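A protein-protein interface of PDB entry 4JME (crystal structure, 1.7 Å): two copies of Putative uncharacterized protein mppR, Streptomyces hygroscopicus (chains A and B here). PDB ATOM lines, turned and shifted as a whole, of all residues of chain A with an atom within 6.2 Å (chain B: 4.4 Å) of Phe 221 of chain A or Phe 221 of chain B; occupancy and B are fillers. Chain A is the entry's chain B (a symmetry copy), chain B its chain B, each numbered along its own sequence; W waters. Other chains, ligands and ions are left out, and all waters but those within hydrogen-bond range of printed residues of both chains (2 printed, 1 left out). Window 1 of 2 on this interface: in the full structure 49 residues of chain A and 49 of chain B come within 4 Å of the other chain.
Water W1 lies within hydrogen-bond range of the backbone carbonyl oxygen of Val 151 of chain B (2.7 Å) and the backbone carbonyl oxygen of Pro 222 of chain A (3.1 Å).
Water W2 lies within hydrogen-bond range of O of Val 151 of chain A (2.7 Å) and O of Pro 222 of chain B (3.1 Å).
Among the printed residues, merely in contact across the chains: Trp 150 of chain A with Met 147 of chain B (3.4 Å), Met 147 of chain A with Trp 150 of chain B (3.4 Å), Tyr 38 of chain A with Pro 222 of chain B (3.5 Å), Phe 221 of chain A with Phe 221 of chain B (3.5 Å), Ser 39 of chain A with Trp 150 of chain B (3.6 Å), Val 151 of chain A with Pro 222 of chain B (3.9 Å), Pro 222 of chain A with Val 151 of chain B (3.9 Å), Ser 39 of chain A with Pro 222 of chain B (3.9 Å), Phe 221 of chain A with Val 151 of chain B (3.9 Å), Val 151 of chain A with Phe 221 of chain B (3.9 Å), Phe 221 of chain A with Trp 150 of chain B (3.9 Å) and Trp 150 of chain A with Phe 221 of chain B (3.9 Å).
Met 147 of chain B touches its own counterpart, Met 147 of chain A.
Met 147 of chain A touches Trp 150 of chain B, and with the chains exchanged Trp 150 of chain A touches Met 147 of chain B.
Trp 150 of chain A touches Phe 221 of chain B, and with the chains exchanged Phe 221 of chain A touches Trp 150 of chain B.
Val 151 of chain A touches Phe 221 of chain B, and with the chains exchanged Phe 221 of chain A touches Val 151 of chain B.
Of the 13 pairs that touch across the chains among the printed residues, 10 have their exchanged pair printed and touching as well.
Phe 221 of chain A touches three residues of chain B.
Of the printed residues of chain B, Pro 222 of chain A touches Val 151 (3.9 Å).
Of the printed residues of chain A, Met 147 of chain B touches Met 147 (3.6 Å) and Trp 150 (3.4 Å).
Of chain A, only Trp 150 (3.9 Å), Val 151 (3.9 Å) and Phe 221 (3.5 Å) come within 4 Å of Phe 221 of chain B.
The nearest residue of chain B that does not touch Phe 221 of chain A is Met 147 of chain B (4.1 Å).
The nearest printed residue of chain A that does not touch Met 147 of chain B is Phe 221 of chain A (4.1 Å).
Of the 13 printed residues of chain A, 7 touch a printed residue of chain B.
Printed residues of chain A that touch a printed residue of chain B: Tyr 38, Ser 39, Met 147, Trp 150, Val 151, Phe 221 and Pro 222.
Hydrophobic or aromatic side chains of chain A that line the printed part of chain B: Tyr 38, Met 147, Trp 150, Val 151, Phe 221 and Pro 222.
Among the printed residues, no Asp or Glu carboxylate lies within 4 Å of a Lys or Arg side-chain nitrogen of the other chain.
The side-chain sulfur (SD) of Met 147 of chain B lies close to the side-chain sulfur (SD) of Met 147 of chain A, 3.6 Å away.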
ATOM      1  N   TYR A  38     -24.383  -4.764 -10.478  1.00  0.00           N
ATOM      2  CA  TYR A  38     -24.023  -4.453 -11.862  1.00  0.00           C
ATOM      3  C   TYR A  38     -22.528  -4.644 -12.094  1.00  0.00           C
ATOM      4  O   TYR A  38     -22.097  -5.077 -13.162  1.00  0.00           O
ATOM      5  CB  TYR A  38     -24.416  -3.022 -12.201  1.00  0.00           C
ATOM      6  CG  TYR A  38     -24.008  -2.627 -13.594  1.00  0.00           C
ATOM      7  CD1 TYR A  38     -24.624  -3.199 -14.706  1.00  0.00           C
ATOM      8  CD2 TYR A  38     -23.008  -1.686 -13.803  1.00  0.00           C
ATOM      9  CE1 TYR A  38     -24.238  -2.846 -15.981  1.00  0.00           C
ATOM     10  CE2 TYR A  38     -22.616  -1.335 -15.060  1.00  0.00           C
ATOM     11  CZ  TYR A  38     -23.241  -1.905 -16.147  1.00  0.00           C
ATOM     12  OH  TYR A  38     -22.849  -1.541 -17.409  1.00  0.00           O
ATOM     13  N   SER A  39     -21.749  -4.330 -11.070  1.00  0.00           N
ATOM     14  CA  SER A  39     -20.297  -4.478 -11.087  1.00  0.00           C
ATOM     15  C   SER A  39     -19.813  -4.847  -9.677  1.00  0.00           C
ATOM     16  O   SER A  39     -20.601  -4.864  -8.735  1.00  0.00           O
ATOM     17  CB  SER A  39     -19.609  -3.180 -11.534  1.00  0.00           C
ATOM     18  OG  SER A  39     -19.503  -2.209 -10.497  1.00  0.00           O
ATOM     19  N   MET A 147     -13.072   3.232 -14.924  1.00  0.00           N
ATOM     20  CA  MET A 147     -13.532   1.860 -15.030  1.00  0.00           C
ATOM     21  C   MET A 147     -14.706   1.756 -16.013  1.00  0.00           C
ATOM     22  O   MET A 147     -14.802   0.784 -16.779  1.00  0.00           O
ATOM     23  CB  MET A 147     -13.942   1.333 -13.656  1.00  0.00           C
ATOM     24  CG  MET A 147     -14.289  -0.140 -13.662  1.00  0.00           C
ATOM     25  SD  MET A 147     -12.859  -1.210 -13.952  1.00  0.00           S
ATOM     26  CE  MET A 147     -11.923  -0.954 -12.432  1.00  0.00           C
ATOM     27  N   TRP A 150     -13.542   1.348 -19.486  1.00  0.00           N
ATOM     28  CA  TRP A 150     -13.143  -0.012 -19.883  1.00  0.00           C
ATOM     29  C   TRP A 150     -14.363  -0.902 -20.192  1.00  0.00           C
ATOM     30  O   TRP A 150     -14.310  -1.772 -21.081  1.00  0.00           O
ATOM     31  CB  TRP A 150     -12.249  -0.658 -18.825  1.00  0.00           C
ATOM     32  CG  TRP A 150     -10.825  -0.136 -18.858  1.00  0.00           C
ATOM     33  CD1 TRP A 150     -10.436   1.176 -18.932  1.00  0.00           C
ATOM     34  CD2 TRP A 150      -9.621  -0.908 -18.851  1.00  0.00           C
ATOM     35  NE1 TRP A 150      -9.070   1.259 -18.956  1.00  0.00           N
ATOM     36  CE2 TRP A 150      -8.542  -0.003 -18.900  1.00  0.00           C
ATOM     37  CE3 TRP A 150      -9.346  -2.271 -18.797  1.00  0.00           C
ATOM     38  CZ2 TRP A 150      -7.212  -0.422 -18.891  1.00  0.00           C
ATOM     39  CZ3 TRP A 150      -8.020  -2.684 -18.796  1.00  0.00           C
ATOM     40  CH2 TRP A 150      -6.973  -1.766 -18.846  1.00  0.00           C
ATOM     41  N   VAL A 151     -15.467  -0.665 -19.492  1.00  0.00           N
ATOM     42  CA  VAL A 151     -16.692  -1.416 -19.757  1.00  0.00           C
ATOM     43  C   VAL A 151     -17.139  -1.212 -21.207  1.00  0.00           C
ATOM     44  O   VAL A 151     -17.653  -2.148 -21.837  1.00  0.00           O
ATOM     45  CB  VAL A 151     -17.827  -1.002 -18.793  1.00  0.00           C
ATOM     46  CG1 VAL A 151     -19.169  -1.575 -19.233  1.00  0.00           C
ATOM     47  CG2 VAL A 151     -17.500  -1.435 -17.384  1.00  0.00           C
ATOM     48  N   GLN A 152     -16.949   0.008 -21.711  1.00  0.00           N
ATOM     49  CA  GLN A 152     -17.363   0.394 -23.079  1.00  0.00           C
ATOM     50  C   GLN A 152     -16.293   0.122 -24.108  1.00  0.00           C
ATOM     51  O   GLN A 152     -16.516   0.330 -25.304  1.00  0.00           O
ATOM     52  CB  GLN A 152     -17.630   1.895 -23.190  1.00  0.00           C
ATOM     53  CG  GLN A 152     -18.600   2.510 -22.296  1.00  0.00           C
ATOM     54  CD  GLN A 152     -18.254   3.995 -22.036  1.00  0.00           C
ATOM     55  OE1 GLN A 152     -17.961   4.785 -22.948  1.00  0.00           O
ATOM     56  NE2 GLN A 152     -18.282   4.360 -20.788  1.00  0.00           N
ATOM     57  N   LEU A 219     -13.792  -3.966 -27.174  1.00  0.00           N
ATOM     58  CA  LEU A 219     -14.052  -4.532 -25.846  1.00  0.00           C
ATOM     59  C   LEU A 219     -13.119  -5.681 -25.609  1.00  0.00           C
ATOM     60  O   LEU A 219     -13.208  -6.730 -26.272  1.00  0.00           O
ATOM     61  CB  LEU A 219     -15.466  -5.103 -25.732  1.00  0.00           C
ATOM     62  CG  LEU A 219     -16.683  -4.206 -25.790  1.00  0.00           C
ATOM     63  CD1 LEU A 219     -17.926  -5.057 -25.581  1.00  0.00           C
ATOM     64  CD2 LEU A 219     -16.597  -3.098 -24.747  1.00  0.00           C
ATOM     65  N   VAL A 220     -12.215  -5.517 -24.655  1.00  0.00           N
ATOM     66  CA  VAL A 220     -11.384  -6.645 -24.292  1.00  0.00           C
ATOM     67  C   VAL A 220     -10.868  -6.426 -22.872  1.00  0.00           C
ATOM     68  O   VAL A 220     -10.622  -5.289 -22.447  1.00  0.00           O
ATOM     69  CB  VAL A 220     -10.237  -6.829 -25.309  1.00  0.00           C
ATOM     70  CG1 VAL A 220      -9.257  -5.660 -25.237  1.00  0.00           C
ATOM     71  CG2 VAL A 220      -9.523  -8.155 -25.096  1.00  0.00           C
ATOM     72  N   PHE A 221     -10.756  -7.523 -22.141  1.00  0.00           N
ATOM     73  CA  PHE A 221     -10.352  -7.462 -20.734  1.00  0.00           C
ATOM     74  C   PHE A 221      -9.364  -8.605 -20.534  1.00  0.00           C
ATOM     75  O   PHE A 221      -9.536  -9.681 -21.094  1.00  0.00           O
ATOM     76  CB  PHE A 221     -11.603  -7.592 -19.843  1.00  0.00           C
ATOM     77  CG  PHE A 221     -11.405  -7.116 -18.440  1.00  0.00           C
ATOM     78  CD1 PHE A 221     -11.131  -5.785 -18.176  1.00  0.00           C
ATOM     79  CD2 PHE A 221     -11.501  -7.998 -17.377  1.00  0.00           C
ATOM     80  CE1 PHE A 221     -10.941  -5.349 -16.868  1.00  0.00           C
ATOM     81  CE2 PHE A 221     -11.319  -7.561 -16.075  1.00  0.00           C
ATOM     82  CZ  PHE A 221     -11.035  -6.247 -15.824  1.00  0.00           C
ATOM     83  N   PRO A 222      -8.299  -8.382 -19.755  1.00  0.00           N
ATOM     84  CA  PRO A 222      -7.280  -9.436 -19.689  1.00  0.00           C
ATOM     85  C   PRO A 222      -7.821 -10.738 -19.123  1.00  0.00           C
ATOM     86  O   PRO A 222      -8.732 -10.701 -18.294  1.00  0.00           O
ATOM     87  CB  PRO A 222      -6.234  -8.844 -18.731  1.00  0.00           C
ATOM     88  CG  PRO A 222      -6.419  -7.415 -18.793  1.00  0.00           C
ATOM     89  CD  PRO A 222      -7.898  -7.176 -19.023  1.00  0.00           C
ATOM     90  N   GLU A 223      -7.281 -11.866 -19.575  1.00  0.00           N
ATOM     91  CA  GLU A 223      -7.679 -13.177 -19.077  1.00  0.00           C
ATOM     92  C   GLU A 223      -6.819 -13.562 -17.883  1.00  0.00           C
ATOM     93  O   GLU A 223      -5.595 -13.628 -17.970  1.00  0.00           O
ATOM     94  CB  GLU A 223      -7.560 -14.258 -20.168  1.00  0.00           C
ATOM     95  CG  GLU A 223      -8.832 -14.461 -20.990  1.00  0.00           C
ATOM     96  CD  GLU A 223      -8.737 -15.637 -21.948  1.00  0.00           C
ATOM     97  OE1 GLU A 223      -7.605 -16.062 -22.266  1.00  0.00           O
ATOM     98  OE2 GLU A 223      -9.797 -16.140 -22.385  1.00  0.00           O
ATOM     99  N   PRO A 231      -8.236 -14.192 -24.785  1.00  0.00           N
ATOM    100  CA  PRO A 231      -9.189 -13.081 -24.880  1.00  0.00           C
ATOM    101  C   PRO A 231      -9.958 -13.094 -26.198  1.00  0.00           C
ATOM    102  O   PRO A 231      -9.400 -13.486 -27.224  1.00  0.00           O
ATOM    103  CB  PRO A 231      -8.289 -11.844 -24.803  1.00  0.00           C
ATOM    104  CG  PRO A 231      -7.111 -12.293 -24.016  1.00  0.00           C
ATOM    105  CD  PRO A 231      -6.895 -13.736 -24.385  1.00  0.00           C
ATOM    106  N   ARG A 232     -11.225 -12.692 -26.162  1.00  0.00           N
ATOM    107  CA  ARG A 232     -12.017 -12.585 -27.383  1.00  0.00           C
ATOM    108  C   ARG A 232     -12.466 -11.127 -27.549  1.00  0.00           C
ATOM    109  O   ARG A 232     -13.477 -10.703 -27.004  1.00  0.00           O
ATOM    110  CB  ARG A 232     -13.194 -13.585 -27.384  1.00  0.00           C
ATOM    111  CG  ARG A 232     -14.616 -13.013 -27.184  1.00  0.00           C
ATOM    112  CD  ARG A 232     -15.659 -13.760 -28.018  1.00  0.00           C
ATOM    113  NE  ARG A 232     -15.678 -15.208 -27.786  1.00  0.00           N
ATOM    114  CZ  ARG A 232     -16.233 -16.091 -28.615  1.00  0.00           C
ATOM    115  NH1 ARG A 232     -16.810 -15.685 -29.745  1.00  0.00           N
ATOM    116  NH2 ARG A 232     -16.203 -17.387 -28.325  1.00  0.00           N
ATOM    117  N   MET B 147      -7.289  -1.310 -11.316  1.00  0.00           N
ATOM    118  CA  MET B 147      -7.721  -2.075 -12.471  1.00  0.00           C
ATOM    119  C   MET B 147      -7.191  -3.513 -12.397  1.00  0.00           C
ATOM    120  O   MET B 147      -7.898  -4.465 -12.765  1.00  0.00           O
ATOM    121  CB  MET B 147      -7.249  -1.401 -13.758  1.00  0.00           C
ATOM    122  CG  MET B 147      -7.791  -2.058 -15.008  1.00  0.00           C
ATOM    123  SD  MET B 147      -9.576  -1.835 -15.218  1.00  0.00           S
ATOM    124  CE  MET B 147      -9.664  -0.063 -15.542  1.00  0.00           C
ATOM    125  N   TRP B 150      -9.436  -5.695 -10.452  1.00  0.00           N
ATOM    126  CA  TRP B 150     -10.617  -6.210 -11.160  1.00  0.00           C
ATOM    127  C   TRP B 150     -10.266  -7.398 -12.078  1.00  0.00           C
ATOM    128  O   TRP B 150     -11.071  -8.332 -12.251  1.00  0.00           O
ATOM    129  CB  TRP B 150     -11.320  -5.103 -11.947  1.00  0.00           C
ATOM    130  CG  TRP B 150     -12.141  -4.183 -11.063  1.00  0.00           C
ATOM    131  CD1 TRP B 150     -11.745  -3.615  -9.880  1.00  0.00           C
ATOM    132  CD2 TRP B 150     -13.491  -3.760 -11.276  1.00  0.00           C
ATOM    133  NE1 TRP B 150     -12.761  -2.859  -9.362  1.00  0.00           N
ATOM    134  CE2 TRP B 150     -13.843  -2.922 -10.198  1.00  0.00           C
ATOM    135  CE3 TRP B 150     -14.433  -3.995 -12.272  1.00  0.00           C
ATOM    136  CZ2 TRP B 150     -15.095  -2.317 -10.097  1.00  0.00           C
ATOM    137  CZ3 TRP B 150     -15.682  -3.397 -12.163  1.00  0.00           C
ATOM    138  CH2 TRP B 150     -16.002  -2.573 -11.087  1.00  0.00           C
ATOM    139  N   VAL B 151      -9.058  -7.387 -12.630  1.00  0.00           N
ATOM    140  CA  VAL B 151      -8.611  -8.500 -13.466  1.00  0.00           C
ATOM    141  C   VAL B 151      -8.623  -9.805 -12.664  1.00  0.00           C
ATOM    142  O   VAL B 151      -8.945 -10.869 -13.214  1.00  0.00           O
ATOM    143  CB  VAL B 151      -7.197  -8.246 -14.035  1.00  0.00           C
ATOM    144  CG1 VAL B 151      -6.618  -9.502 -14.674  1.00  0.00           C
ATOM    145  CG2 VAL B 151      -7.231  -7.110 -15.029  1.00  0.00           C
ATOM    146  N   VAL B 220     -15.897 -11.128 -12.534  1.00  0.00           N
ATOM    147  CA  VAL B 220     -17.039 -10.745 -13.337  1.00  0.00           C
ATOM    148  C   VAL B 220     -16.857  -9.293 -13.772  1.00  0.00           C
ATOM    149  O   VAL B 220     -16.286  -8.472 -13.042  1.00  0.00           O
ATOM    150  CB  VAL B 220     -18.353 -10.962 -12.557  1.00  0.00           C
ATOM    151  CG1 VAL B 220     -18.444 -10.001 -11.373  1.00  0.00           C
ATOM    152  CG2 VAL B 220     -19.562 -10.822 -13.469  1.00  0.00           C
ATOM    153  N   PHE B 221     -17.309  -9.009 -14.982  1.00  0.00           N
ATOM    154  CA  PHE B 221     -17.131  -7.679 -15.569  1.00  0.00           C
ATOM    155  C   PHE B 221     -18.456  -7.341 -16.244  1.00  0.00           C
ATOM    156  O   PHE B 221     -19.094  -8.206 -16.828  1.00  0.00           O
ATOM    157  CB  PHE B 221     -15.950  -7.715 -16.558  1.00  0.00           C
ATOM    158  CG  PHE B 221     -15.388  -6.369 -16.887  1.00  0.00           C
ATOM    159  CD1 PHE B 221     -14.783  -5.596 -15.910  1.00  0.00           C
ATOM    160  CD2 PHE B 221     -15.454  -5.876 -18.178  1.00  0.00           C
ATOM    161  CE1 PHE B 221     -14.268  -4.342 -16.221  1.00  0.00           C
ATOM    162  CE2 PHE B 221     -14.933  -4.629 -18.487  1.00  0.00           C
ATOM    163  CZ  PHE B 221     -14.350  -3.866 -17.514  1.00  0.00           C
ATOM    164  N   PRO B 222     -18.902  -6.082 -16.149  1.00  0.00           N
ATOM    165  CA  PRO B 222     -20.244  -5.803 -16.672  1.00  0.00           C
ATOM    166  C   PRO B 222     -20.359  -6.070 -18.164  1.00  0.00           C
ATOM    167  O   PRO B 222     -19.368  -5.916 -18.880  1.00  0.00           O
ATOM    168  CB  PRO B 222     -20.417  -4.301 -16.395  1.00  0.00           C
ATOM    169  CG  PRO B 222     -19.510  -4.002 -15.314  1.00  0.00           C
ATOM    170  CD  PRO B 222     -18.313  -4.916 -15.482  1.00  0.00           C
ATOM    171  N   GLU B 223     -21.540  -6.478 -18.618  1.00  0.00           N
ATOM    172  CA  GLU B 223     -21.792  -6.723 -20.033  1.00  0.00           C
ATOM    173  C   GLU B 223     -22.279  -5.446 -20.701  1.00  0.00           C
ATOM    174  O   GLU B 223     -23.287  -4.863 -20.309  1.00  0.00           O
ATOM    175  CB  GLU B 223     -22.829  -7.842 -20.239  1.00  0.00           C
ATOM    176  CG  GLU B 223     -22.226  -9.241 -20.362  1.00  0.00           C
ATOM    177  CD  GLU B 223     -23.254 -10.301 -20.721  1.00  0.00           C
ATOM    178  OE1 GLU B 223     -24.463 -10.059 -20.513  1.00  0.00           O
ATOM    179  OE2 GLU B 223     -22.853 -11.378 -21.218  1.00  0.00           O
HETATM  180  O   HOH W   1     -10.188 -11.134 -15.596  1.00  0.00           O
HETATM  181  O   HOH W   2     -17.610  -4.760 -21.152  1.00  0.00           O
